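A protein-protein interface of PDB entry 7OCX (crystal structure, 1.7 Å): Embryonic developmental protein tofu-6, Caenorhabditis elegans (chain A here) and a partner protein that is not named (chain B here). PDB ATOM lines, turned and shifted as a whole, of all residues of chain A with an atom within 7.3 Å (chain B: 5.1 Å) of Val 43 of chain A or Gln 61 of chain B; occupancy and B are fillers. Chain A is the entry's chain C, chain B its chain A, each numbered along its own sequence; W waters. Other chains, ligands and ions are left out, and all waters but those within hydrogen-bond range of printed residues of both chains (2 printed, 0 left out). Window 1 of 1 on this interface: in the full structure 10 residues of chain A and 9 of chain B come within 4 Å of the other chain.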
ATOM      1  N   TRP A  31       9.950  11.396  27.051  1.00  0.00           N
ATOM      2  CA  TRP A  31      10.054  12.513  26.117  1.00  0.00           C
ATOM      3  C   TRP A  31       9.114  13.657  26.481  1.00  0.00           C
ATOM      4  O   TRP A  31       9.471  14.821  26.295  1.00  0.00           O
ATOM      5  CB  TRP A  31       9.812  12.070  24.684  1.00  0.00           C
ATOM      6  CG  TRP A  31      10.928  11.287  24.128  1.00  0.00           C
ATOM      7  CD1 TRP A  31      10.963   9.934  23.942  1.00  0.00           C
ATOM      8  CD2 TRP A  31      12.222  11.778  23.729  1.00  0.00           C
ATOM      9  NE1 TRP A  31      12.170   9.556  23.418  1.00  0.00           N
ATOM     10  CE2 TRP A  31      12.968  10.665  23.294  1.00  0.00           C
ATOM     11  CE3 TRP A  31      12.817  13.048  23.695  1.00  0.00           C
ATOM     12  CZ2 TRP A  31      14.267  10.784  22.804  1.00  0.00           C
ATOM     13  CZ3 TRP A  31      14.118  13.168  23.235  1.00  0.00           C
ATOM     14  CH2 TRP A  31      14.837  12.044  22.806  1.00  0.00           C
ATOM     15  N   LEU A  33       8.341  14.538  29.566  1.00  0.00           N
ATOM     16  CA  LEU A  33       9.065  15.164  30.669  1.00  0.00           C
ATOM     17  C   LEU A  33      10.246  15.976  30.154  1.00  0.00           C
ATOM     18  O   LEU A  33      10.481  17.115  30.583  1.00  0.00           O
ATOM     19  CB  LEU A  33       9.530  14.067  31.630  1.00  0.00           C
ATOM     20  CG  LEU A  33      10.218  14.519  32.915  1.00  0.00           C
ATOM     21  CD1 LEU A  33       9.318  15.421  33.735  1.00  0.00           C
ATOM     22  CD2 LEU A  33      10.646  13.310  33.730  1.00  0.00           C
ATOM     23  N   PHE A  34      11.010  15.396  29.230  1.00  0.00           N
ATOM     24  CA  PHE A  34      12.117  16.124  28.622  1.00  0.00           C
ATOM     25  C   PHE A  34      11.637  17.442  28.016  1.00  0.00           C
ATOM     26  O   PHE A  34      12.271  18.491  28.190  1.00  0.00           O
ATOM     27  CB  PHE A  34      12.788  15.228  27.571  1.00  0.00           C
ATOM     28  CG  PHE A  34      13.650  15.973  26.602  1.00  0.00           C
ATOM     29  CD1 PHE A  34      14.959  16.299  26.927  1.00  0.00           C
ATOM     30  CD2 PHE A  34      13.145  16.346  25.364  1.00  0.00           C
ATOM     31  CE1 PHE A  34      15.756  16.998  26.041  1.00  0.00           C
ATOM     32  CE2 PHE A  34      13.927  17.051  24.473  1.00  0.00           C
ATOM     33  CZ  PHE A  34      15.242  17.382  24.809  1.00  0.00           C
ATOM     34  N   HIS A  35      10.508  17.402  27.297  1.00  0.00           N
ATOM     35  CA  HIS A  35      10.053  18.604  26.594  1.00  0.00           C
ATOM     36  C   HIS A  35       9.747  19.723  27.585  1.00  0.00           C
ATOM     37  O   HIS A  35      10.014  20.900  27.316  1.00  0.00           O
ATOM     38  CB  HIS A  35       8.807  18.345  25.730  1.00  0.00           C
ATOM     39  CG  HIS A  35       9.048  17.494  24.516  1.00  0.00           C
ATOM     40  ND1 HIS A  35      10.233  17.502  23.812  1.00  0.00           N
ATOM     41  CD2 HIS A  35       8.209  16.679  23.825  1.00  0.00           C
ATOM     42  CE1 HIS A  35      10.143  16.670  22.787  1.00  0.00           C
ATOM     43  NE2 HIS A  35       8.920  16.168  22.763  1.00  0.00           N
ATOM     44  N   VAL A  36       9.148  19.379  28.724  1.00  0.00           N
ATOM     45  CA  VAL A  36       8.835  20.401  29.712  1.00  0.00           C
ATOM     46  C   VAL A  36      10.104  21.071  30.210  1.00  0.00           C
ATOM     47  O   VAL A  36      10.153  22.300  30.351  1.00  0.00           O
ATOM     48  CB  VAL A  36       8.028  19.813  30.881  1.00  0.00           C
ATOM     49  CG1 VAL A  36       8.004  20.815  32.042  1.00  0.00           C
ATOM     50  CG2 VAL A  36       6.642  19.484  30.398  1.00  0.00           C
ATOM     51  N   PHE A  37      11.139  20.278  30.509  1.00  0.00           N
ATOM     52  CA  PHE A  37      12.345  20.855  31.092  1.00  0.00           C
ATOM     53  C   PHE A  37      13.264  21.457  30.048  1.00  0.00           C
ATOM     54  O   PHE A  37      14.002  22.399  30.353  1.00  0.00           O
ATOM     55  CB  PHE A  37      13.050  19.813  31.962  1.00  0.00           C
ATOM     56  CG  PHE A  37      12.392  19.675  33.283  1.00  0.00           C
ATOM     57  CD1 PHE A  37      11.241  18.934  33.425  1.00  0.00           C
ATOM     58  CD2 PHE A  37      12.861  20.407  34.364  1.00  0.00           C
ATOM     59  CE1 PHE A  37      10.586  18.885  34.638  1.00  0.00           C
ATOM     60  CE2 PHE A  37      12.220  20.346  35.584  1.00  0.00           C
ATOM     61  CZ  PHE A  37      11.079  19.584  35.716  1.00  0.00           C
ATOM     62  N   GLN A  38      13.195  20.997  28.809  1.00  0.00           N
ATOM     63  CA  GLN A  38      13.990  21.624  27.767  1.00  0.00           C
ATOM     64  C   GLN A  38      13.672  23.108  27.590  1.00  0.00           C
ATOM     65  O   GLN A  38      14.514  23.860  27.086  1.00  0.00           O
ATOM     66  CB  GLN A  38      13.764  20.912  26.444  1.00  0.00           C
ATOM     67  CG  GLN A  38      14.956  20.936  25.563  1.00  0.00           C
ATOM     68  CD  GLN A  38      14.560  20.804  24.115  1.00  0.00           C
ATOM     69  OE1 GLN A  38      13.395  20.556  23.798  1.00  0.00           O
ATOM     70  NE2 GLN A  38      15.524  20.983  23.223  1.00  0.00           N
ATOM     71  N   ASN A  39      12.449  23.540  27.912  1.00  0.00           N
ATOM     72  CA  ASN A  39      12.129  24.961  27.765  1.00  0.00           C
ATOM     73  C   ASN A  39      12.968  25.853  28.669  1.00  0.00           C
ATOM     74  O   ASN A  39      13.028  27.067  28.440  1.00  0.00           O
ATOM     75  CB  ASN A  39      10.651  25.230  28.055  1.00  0.00           C
ATOM     76  CG  ASN A  39       9.704  24.624  27.042  1.00  0.00           C
ATOM     77  OD1 ASN A  39       9.989  24.574  25.842  1.00  0.00           O
ATOM     78  ND2 ASN A  39       8.576  24.121  27.529  1.00  0.00           N
ATOM     79  N   PHE A  40      13.586  25.295  29.704  1.00  0.00           N
ATOM     80  CA  PHE A  40      14.401  26.048  30.651  1.00  0.00           C
ATOM     81  C   PHE A  40      15.887  25.951  30.372  1.00  0.00           C
ATOM     82  O   PHE A  40      16.667  26.705  30.970  1.00  0.00           O
ATOM     83  CB  PHE A  40      14.111  25.560  32.074  1.00  0.00           C
ATOM     84  CG  PHE A  40      12.666  25.653  32.440  1.00  0.00           C
ATOM     85  CD1 PHE A  40      11.897  24.514  32.554  1.00  0.00           C
ATOM     86  CD2 PHE A  40      12.073  26.889  32.659  1.00  0.00           C
ATOM     87  CE1 PHE A  40      10.560  24.597  32.876  1.00  0.00           C
ATOM     88  CE2 PHE A  40      10.735  26.982  32.989  1.00  0.00           C
ATOM     89  CZ  PHE A  40       9.977  25.832  33.094  1.00  0.00           C
ATOM     90  N   GLY A  41      16.297  25.056  29.494  1.00  0.00           N
ATOM     91  CA  GLY A  41      17.702  24.895  29.189  1.00  0.00           C
ATOM     92  C   GLY A  41      17.996  23.491  28.702  1.00  0.00           C
ATOM     93  O   GLY A  41      17.105  22.657  28.543  1.00  0.00           O
ATOM     94  N   LYS A  42      19.273  23.255  28.447  1.00  0.00           N
ATOM     95  CA  LYS A  42      19.691  21.951  27.994  1.00  0.00           C
ATOM     96  C   LYS A  42      19.514  20.928  29.115  1.00  0.00           C
ATOM     97  O   LYS A  42      19.652  21.230  30.302  1.00  0.00           O
ATOM     98  CB  LYS A  42      21.136  21.987  27.501  1.00  0.00           C
ATOM     99  CG  LYS A  42      21.369  22.880  26.275  1.00  0.00           C
ATOM    100  CD  LYS A  42      22.864  22.939  25.943  1.00  0.00           C
ATOM    101  CE  LYS A  42      23.155  23.750  24.688  1.00  0.00           C
ATOM    102  NZ  LYS A  42      22.852  25.161  24.856  1.00  0.00           N
ATOM    103  N   VAL A  43      19.152  19.713  28.725  1.00  0.00           N
ATOM    104  CA  VAL A  43      18.845  18.629  29.653  1.00  0.00           C
ATOM    105  C   VAL A  43      19.888  17.538  29.511  1.00  0.00           C
ATOM    106  O   VAL A  43      20.125  17.039  28.408  1.00  0.00           O
ATOM    107  CB  VAL A  43      17.439  18.054  29.393  1.00  0.00           C
ATOM    108  CG1 VAL A  43      17.163  16.875  30.314  1.00  0.00           C
ATOM    109  CG2 VAL A  43      16.363  19.144  29.554  1.00  0.00           C
ATOM    110  N   SER A  44      20.483  17.122  30.630  1.00  0.00           N
ATOM    111  CA  SER A  44      21.478  16.058  30.570  1.00  0.00           C
ATOM    112  C   SER A  44      20.874  14.668  30.684  1.00  0.00           C
ATOM    113  O   SER A  44      21.334  13.734  30.019  1.00  0.00           O
ATOM    114  CB  SER A  44      22.506  16.232  31.693  1.00  0.00           C
ATOM    115  OG  SER A  44      23.312  15.077  31.806  1.00  0.00           O
ATOM    116  N   TYR A  45      19.865  14.498  31.539  1.00  0.00           N
ATOM    117  CA  TYR A  45      19.223  13.205  31.722  1.00  0.00           C
ATOM    118  C   TYR A  45      17.792  13.387  32.194  1.00  0.00           C
ATOM    119  O   TYR A  45      17.477  14.331  32.909  1.00  0.00           O
ATOM    120  CB  TYR A  45      19.915  12.293  32.736  1.00  0.00           C
ATOM    121  CG  TYR A  45      19.442  10.848  32.658  1.00  0.00           C
ATOM    122  CD1 TYR A  45      19.203  10.238  31.423  1.00  0.00           C
ATOM    123  CD2 TYR A  45      19.259  10.086  33.811  1.00  0.00           C
ATOM    124  CE1 TYR A  45      18.775   8.922  31.341  1.00  0.00           C
ATOM    125  CE2 TYR A  45      18.842   8.762  33.738  1.00  0.00           C
ATOM    126  CZ  TYR A  45      18.603   8.189  32.500  1.00  0.00           C
ATOM    127  OH  TYR A  45      18.190   6.878  32.434  1.00  0.00           O
ATOM    128  N   CYS A  46      16.967  12.401  31.867  1.00  0.00           N
ATOM    129  CA  CYS A  46      15.535  12.475  32.042  1.00  0.00           C
ATOM    130  C   CYS A  46      14.981  11.063  32.124  1.00  0.00           C
ATOM    131  O   CYS A  46      15.191  10.279  31.199  1.00  0.00           O
ATOM    132  CB  CYS A  46      14.953  13.225  30.846  1.00  0.00           C
ATOM    133  SG  CYS A  46      13.283  13.500  30.946  1.00  0.00           S
ATOM    134  N   PHE A  61      12.859  12.011  37.384  1.00  0.00           N
ATOM    135  CA  PHE A  61      14.150  12.576  37.720  1.00  0.00           C
ATOM    136  C   PHE A  61      14.611  13.309  36.475  1.00  0.00           C
ATOM    137  O   PHE A  61      14.472  12.797  35.362  1.00  0.00           O
ATOM    138  CB  PHE A  61      15.136  11.490  38.100  1.00  0.00           C
ATOM    139  CG  PHE A  61      16.505  11.973  38.260  1.00  0.00           C
ATOM    140  CD1 PHE A  61      16.845  12.751  39.369  1.00  0.00           C
ATOM    141  CD2 PHE A  61      17.469  11.647  37.342  1.00  0.00           C
ATOM    142  CE1 PHE A  61      18.133  13.209  39.542  1.00  0.00           C
ATOM    143  CE2 PHE A  61      18.739  12.071  37.523  1.00  0.00           C
ATOM    144  CZ  PHE A  61      19.082  12.861  38.632  1.00  0.00           C
ATOM    145  N   VAL A  62      15.105  14.521  36.663  1.00  0.00           N
ATOM    146  CA  VAL A  62      15.627  15.334  35.576  1.00  0.00           C
ATOM    147  C   VAL A  62      16.920  15.974  36.048  1.00  0.00           C
ATOM    148  O   VAL A  62      16.961  16.531  37.145  1.00  0.00           O
ATOM    149  CB  VAL A  62      14.639  16.434  35.142  1.00  0.00           C
ATOM    150  CG1 VAL A  62      15.277  17.322  34.099  1.00  0.00           C
ATOM    151  CG2 VAL A  62      13.410  15.816  34.583  1.00  0.00           C
ATOM    152  N   ASN A  63      17.970  15.906  35.221  1.00  0.00           N
ATOM    153  CA  ASN A  63      19.220  16.603  35.499  1.00  0.00           C
ATOM    154  C   ASN A  63      19.437  17.597  34.364  1.00  0.00           C
ATOM    155  O   ASN A  63      19.444  17.207  33.189  1.00  0.00           O
ATOM    156  CB  ASN A  63      20.391  15.609  35.652  1.00  0.00           C
ATOM    157  CG  ASN A  63      21.611  16.249  36.312  1.00  0.00           C
ATOM    158  OD1 ASN A  63      21.641  16.387  37.540  1.00  0.00           O
ATOM    159  ND2 ASN A  63      22.658  16.534  35.536  1.00  0.00           N
ATOM    160  N   MET A  64      19.605  18.868  34.715  1.00  0.00           N
ATOM    161  CA  MET A  64      19.911  19.848  33.694  1.00  0.00           C
ATOM    162  C   MET A  64      21.390  19.779  33.331  1.00  0.00           C
ATOM    163  O   MET A  64      22.215  19.217  34.055  1.00  0.00           O
ATOM    164  CB  MET A  64      19.527  21.251  34.145  1.00  0.00           C
ATOM    165  CG  MET A  64      18.081  21.448  34.573  1.00  0.00           C
ATOM    166  SD  MET A  64      16.881  20.963  33.353  1.00  0.00           S
ATOM    167  CE  MET A  64      17.023  22.324  32.175  1.00  0.00           C
ATOM    168  N   MET A  65      21.718  20.332  32.171  1.00  0.00           N
ATOM    169  CA  MET A  65      23.103  20.291  31.726  1.00  0.00           C
ATOM    170  C   MET A  65      24.005  21.165  32.585  1.00  0.00           C
ATOM    171  O   MET A  65      25.218  20.927  32.638  1.00  0.00           O
ATOM    172  CB  MET A  65      23.194  20.725  30.265  1.00  0.00           C
ATOM    173  CG  MET A  65      24.568  20.522  29.720  1.00  0.00           C
ATOM    174  SD  MET A  65      25.019  18.849  29.289  1.00  0.00           S
ATOM    175  CE  MET A  65      23.501  18.154  28.647  1.00  0.00           C
ATOM    176  N   SER A  66      23.449  22.167  33.247  1.00  0.00           N
ATOM    177  CA  SER A  66      24.263  23.078  34.035  1.00  0.00           C
ATOM    178  C   SER A  66      23.431  23.632  35.175  1.00  0.00           C
ATOM    179  O   SER A  66      22.200  23.625  35.132  1.00  0.00           O
ATOM    180  CB  SER A  66      24.829  24.184  33.140  1.00  0.00           C
ATOM    181  OG  SER A  66      23.822  25.126  32.806  1.00  0.00           O
ATOM    182  N   ASP A  69      21.112  26.315  34.097  1.00  0.00           N
ATOM    183  CA  ASP A  69      19.821  25.821  33.599  1.00  0.00           C
ATOM    184  C   ASP A  69      18.896  25.445  34.749  1.00  0.00           C
ATOM    185  O   ASP A  69      17.692  25.734  34.714  1.00  0.00           O
ATOM    186  CB  ASP A  69      20.018  24.598  32.705  1.00  0.00           C
ATOM    187  CG  ASP A  69      20.787  24.893  31.436  1.00  0.00           C
ATOM    188  OD1 ASP A  69      20.696  26.028  30.934  1.00  0.00           O
ATOM    189  OD2 ASP A  69      21.499  23.968  30.966  1.00  0.00           O
ATOM    190  N   TYR B  36      27.669  18.733  25.485  1.00  0.00           N
ATOM    191  CA  TYR B  36      27.124  17.382  25.639  1.00  0.00           C
ATOM    192  C   TYR B  36      28.220  16.409  26.042  1.00  0.00           C
ATOM    193  O   TYR B  36      29.369  16.517  25.604  1.00  0.00           O
ATOM    194  CB  TYR B  36      26.395  16.884  24.357  1.00  0.00           C
ATOM    195  CG  TYR B  36      25.286  17.842  24.025  1.00  0.00           C
ATOM    196  CD1 TYR B  36      24.172  17.927  24.854  1.00  0.00           C
ATOM    197  CD2 TYR B  36      25.384  18.735  22.964  1.00  0.00           C
ATOM    198  CE1 TYR B  36      23.194  18.895  24.641  1.00  0.00           C
ATOM    199  CE2 TYR B  36      24.382  19.674  22.723  1.00  0.00           C
ATOM    200  CZ  TYR B  36      23.290  19.742  23.561  1.00  0.00           C
ATOM    201  OH  TYR B  36      22.320  20.668  23.338  1.00  0.00           O
ATOM    202  N   PHE B  57      18.762  11.683  24.802  1.00  0.00           N
ATOM    203  CA  PHE B  57      18.326  13.075  24.920  1.00  0.00           C
ATOM    204  C   PHE B  57      19.426  14.033  24.486  1.00  0.00           C
ATOM    205  O   PHE B  57      19.153  15.050  23.822  1.00  0.00           O
ATOM    206  CB  PHE B  57      17.900  13.398  26.360  1.00  0.00           C
ATOM    207  CG  PHE B  57      16.841  12.511  26.892  1.00  0.00           C
ATOM    208  CD1 PHE B  57      15.516  12.663  26.498  1.00  0.00           C
ATOM    209  CD2 PHE B  57      17.161  11.494  27.765  1.00  0.00           C
ATOM    210  CE1 PHE B  57      14.527  11.819  26.977  1.00  0.00           C
ATOM    211  CE2 PHE B  57      16.182  10.630  28.228  1.00  0.00           C
ATOM    212  CZ  PHE B  57      14.865  10.799  27.840  1.00  0.00           C
ATOM    213  N   GLN B  58      20.672  13.723  24.864  1.00  0.00           N
ATOM    214  CA  GLN B  58      21.807  14.478  24.371  1.00  0.00           C
ATOM    215  C   GLN B  58      21.996  14.295  22.867  1.00  0.00           C
ATOM    216  O   GLN B  58      22.315  15.274  22.176  1.00  0.00           O
ATOM    217  CB  GLN B  58      23.048  14.106  25.182  1.00  0.00           C
ATOM    218  CG  GLN B  58      22.810  14.405  26.678  1.00  0.00           C
ATOM    219  CD  GLN B  58      24.076  14.545  27.472  1.00  0.00           C
ATOM    220  OE1 GLN B  58      25.135  14.849  26.915  1.00  0.00           O
ATOM    221  NE2 GLN B  58      23.992  14.281  28.780  1.00  0.00           N
ATOM    222  N   VAL B  59      21.724  13.104  22.328  1.00  0.00           N
ATOM    223  CA  VAL B  59      21.768  12.935  20.871  1.00  0.00           C
ATOM    224  C   VAL B  59      20.778  13.864  20.199  1.00  0.00           C
ATOM    225  O   VAL B  59      21.112  14.577  19.245  1.00  0.00           O
ATOM    226  CB  VAL B  59      21.496  11.473  20.474  1.00  0.00           C
ATOM    227  CG1 VAL B  59      21.343  11.369  18.946  1.00  0.00           C
ATOM    228  CG2 VAL B  59      22.628  10.580  20.958  1.00  0.00           C
ATOM    229  N   TYR B  60      19.536  13.853  20.676  1.00  0.00           N
ATOM    230  CA  TYR B  60      18.489  14.681  20.092  1.00  0.00           C
ATOM    231  C   TYR B  60      18.884  16.154  20.102  1.00  0.00           C
ATOM    232  O   TYR B  60      18.659  16.881  19.123  1.00  0.00           O
ATOM    233  CB  TYR B  60      17.188  14.468  20.875  1.00  0.00           C
ATOM    234  CG  TYR B  60      16.110  15.444  20.524  1.00  0.00           C
ATOM    235  CD1 TYR B  60      15.347  15.278  19.372  1.00  0.00           C
ATOM    236  CD2 TYR B  60      15.861  16.557  21.318  1.00  0.00           C
ATOM    237  CE1 TYR B  60      14.365  16.200  19.026  1.00  0.00           C
ATOM    238  CE2 TYR B  60      14.881  17.471  20.973  1.00  0.00           C
ATOM    239  CZ  TYR B  60      14.143  17.293  19.832  1.00  0.00           C
ATOM    240  OH  TYR B  60      13.180  18.223  19.501  1.00  0.00           O
ATOM    241  N   GLN B  61      19.401  16.620  21.230  1.00  0.00           N
ATOM    242  CA  GLN B  61      19.720  18.039  21.362  1.00  0.00           C
ATOM    243  C   GLN B  61      20.945  18.396  20.529  1.00  0.00           C
ATOM    244  O   GLN B  61      20.995  19.480  19.925  1.00  0.00           O
ATOM    245  CB  GLN B  61      19.927  18.402  22.829  1.00  0.00           C
ATOM    246  CG  GLN B  61      18.692  18.214  23.697  1.00  0.00           C
ATOM    247  CD  GLN B  61      19.006  18.383  25.169  1.00  0.00           C
ATOM    248  OE1 GLN B  61      18.908  19.476  25.730  1.00  0.00           O
ATOM    249  NE2 GLN B  61      19.451  17.299  25.786  1.00  0.00           N
ATOM    250  N   ALA B  62      21.901  17.473  20.418  1.00  0.00           N
ATOM    251  CA  ALA B  62      23.087  17.738  19.607  1.00  0.00           C
ATOM    252  C   ALA B  62      22.728  17.809  18.135  1.00  0.00           C
ATOM    253  O   ALA B  62      23.274  18.629  17.384  1.00  0.00           O
ATOM    254  CB  ALA B  62      24.154  16.666  19.813  1.00  0.00           C
ATOM    255  N   VAL B  63      21.823  16.941  17.683  1.00  0.00           N
ATOM    256  CA  VAL B  63      21.392  17.014  16.290  1.00  0.00           C
ATOM    257  C   VAL B  63      20.735  18.354  16.008  1.00  0.00           C
ATOM    258  O   VAL B  63      21.019  19.014  14.998  1.00  0.00           O
ATOM    259  CB  VAL B  63      20.446  15.840  15.944  1.00  0.00           C
ATOM    260  CG1 VAL B  63      19.799  16.099  14.583  1.00  0.00           C
ATOM    261  CG2 VAL B  63      21.209  14.580  15.952  1.00  0.00           C
ATOM    262  N   GLN B  64      19.835  18.785  16.896  1.00  0.00           N
ATOM    263  CA  GLN B  64      19.161  20.053  16.693  1.00  0.00           C
ATOM    264  C   GLN B  64      20.131  21.230  16.745  1.00  0.00           C
ATOM    265  O   GLN B  64      19.960  22.212  16.003  1.00  0.00           O
ATOM    266  CB  GLN B  64      18.038  20.243  17.717  1.00  0.00           C
ATOM    267  CG  GLN B  64      16.989  19.150  17.618  1.00  0.00           C
ATOM    268  CD  GLN B  64      16.325  19.155  16.254  1.00  0.00           C
ATOM    269  OE1 GLN B  64      16.307  18.127  15.574  1.00  0.00           O
ATOM    270  NE2 GLN B  64      15.754  20.294  15.855  1.00  0.00           N
ATOM    271  N   ASP B  65      21.114  21.171  17.643  1.00  0.00           N
ATOM    272  CA  ASP B  65      22.053  22.287  17.776  1.00  0.00           C
ATOM    273  C   ASP B  65      23.017  22.380  16.592  1.00  0.00           C
ATOM    274  O   ASP B  65      23.376  23.493  16.166  1.00  0.00           O
ATOM    275  CB  ASP B  65      22.904  22.152  19.041  1.00  0.00           C
ATOM    276  CG  ASP B  65      22.149  22.444  20.309  1.00  0.00           C
ATOM    277  OD1 ASP B  65      21.011  22.906  20.238  1.00  0.00           O
ATOM    278  OD2 ASP B  65      22.766  22.306  21.411  1.00  0.00           O
ATOM    279  N   PHE B  66      23.473  21.232  16.081  1.00  0.00           N
ATOM    280  CA  PHE B  66      24.653  21.204  15.226  1.00  0.00           C
ATOM    281  C   PHE B  66      24.405  20.728  13.803  1.00  0.00           C
ATOM    282  O   PHE B  66      25.222  21.032  12.938  1.00  0.00           O
ATOM    283  CB  PHE B  66      25.744  20.318  15.844  1.00  0.00           C
ATOM    284  CG  PHE B  66      26.118  20.728  17.248  1.00  0.00           C
ATOM    285  CD1 PHE B  66      26.485  22.025  17.555  1.00  0.00           C
ATOM    286  CD2 PHE B  66      26.073  19.792  18.271  1.00  0.00           C
ATOM    287  CE1 PHE B  66      26.792  22.378  18.862  1.00  0.00           C
ATOM    288  CE2 PHE B  66      26.385  20.149  19.570  1.00  0.00           C
ATOM    289  CZ  PHE B  66      26.731  21.429  19.863  1.00  0.00           C
HETATM  290  O   HOH W   1      18.161  21.644  24.332  1.00  0.00           O
HETATM  291  O   HOH W   2      25.727  14.761  31.199  1.00  0.00           O
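Val 43 of chain A touches just one residue of chain B: Gln 61.
Gln 61 of chain B touches just these residues of chain A: Phe 34 (3.6 Å), Lys 42 (3.4 Å) and Val 43 (2.7 Å).
Of the printed residues of chain A, Gln 58 of chain B touches Ser 44 and Met 65.
Printed residues of chain B within 4 Å of Trp 31 of chain A: Phe 57 (3.6 Å) and Tyr 60 (3.9 Å).
Printed residues of chain B within 4 Å of Cys 46 of chain A: Phe 57 (3.2 Å).
Of the printed residues of chain B, Lys 42 of chain A touches Tyr 36, Gln 61 and Asp 65.
Of the printed residues of chain B, Met 65 of chain A touches Tyr 36 (3.9 Å) and Gln 58 (3.8 Å).
Of the 11 printed residues of chain B, 6 touch a printed residue of chain A.
Trp 31 of chain A touches Phe 57 of chain B.
Trp 31 of chain A touches Tyr 60 of chain B (CH2 to CB, 3.9 Å).
CD1 of Phe 34 of chain A touches CD1 of Phe 57 of chain B (3.7 Å).
Phe 34 of chain A touches Tyr 60 of chain B (CZ to CD2, 3.6 Å).
Phe 34 of chain A touches Gln 61 of chain B (CE1 to CD, 3.6 Å).
Lys 42 of chain A touches Tyr 36 of chain B.
OE1 of Gln 61 of chain B touches CA of Lys 42 of chain A, 3.4 Å away.
OD2 of Asp 65 of chain B touches CE of Lys 42 of chain A, 3.6 Å away.
Cys 46 of chain A touches Phe 57 of chain B (O to CE2, 3.2 Å).
Met 65 of chain A touches Gln 58 of chain B (CE to CD, 3.8 Å).
The side-chain carboxylate (OD2) of Asp 65 of chain B is in hydrogen-bond range of the side-chain hydroxyl (OH) of Tyr 36 of chain B (2.6 Å).
The backbone carbonyl oxygen (O) of Phe 57 of chain B lies within hydrogen-bond range of the side-chain amide nitrogen (NE2) of Gln 61 of chain B.
The backbone NH (N) of Phe 34 of chain A sits at hydrogen-bond distance from the side-chain sulfur (SG) of Cys 46 of chain A (3.4 Å).
The backbone NH (N) of Met 65 of chain A is in hydrogen-bond range of the backbone carbonyl oxygen (O) of Lys 42 of chain A, 2.9 Å away.
N of Lys 42 of chain A is in hydrogen-bond range of OD2 of Asp 69 of chain A (3.4 Å).
The backbone carbonyl oxygen of Asn 63 of chain A lies within hydrogen-bond range of the backbone NH of Ser 44 of chain A (2.8 Å).
Water W2 bridges the side-chain hydroxyl of Ser 44 of chain A and the side-chain amide nitrogen of Gln 58 of chain B.
Water W1 lies within hydrogen-bond range of OE1 of Gln 61 of chain B (2.7 Å) and NE2 of Gln 38 of chain A (2.9 Å).
NE2 of Gln 58 of chain B lies within hydrogen-bond range of O of Ser 44 of chain A (3.0 Å).
The backbone carbonyl oxygen of Val 43 of chain A sits at hydrogen-bond distance from the side-chain amide nitrogen of Gln 61 of chain B (2.7 Å).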
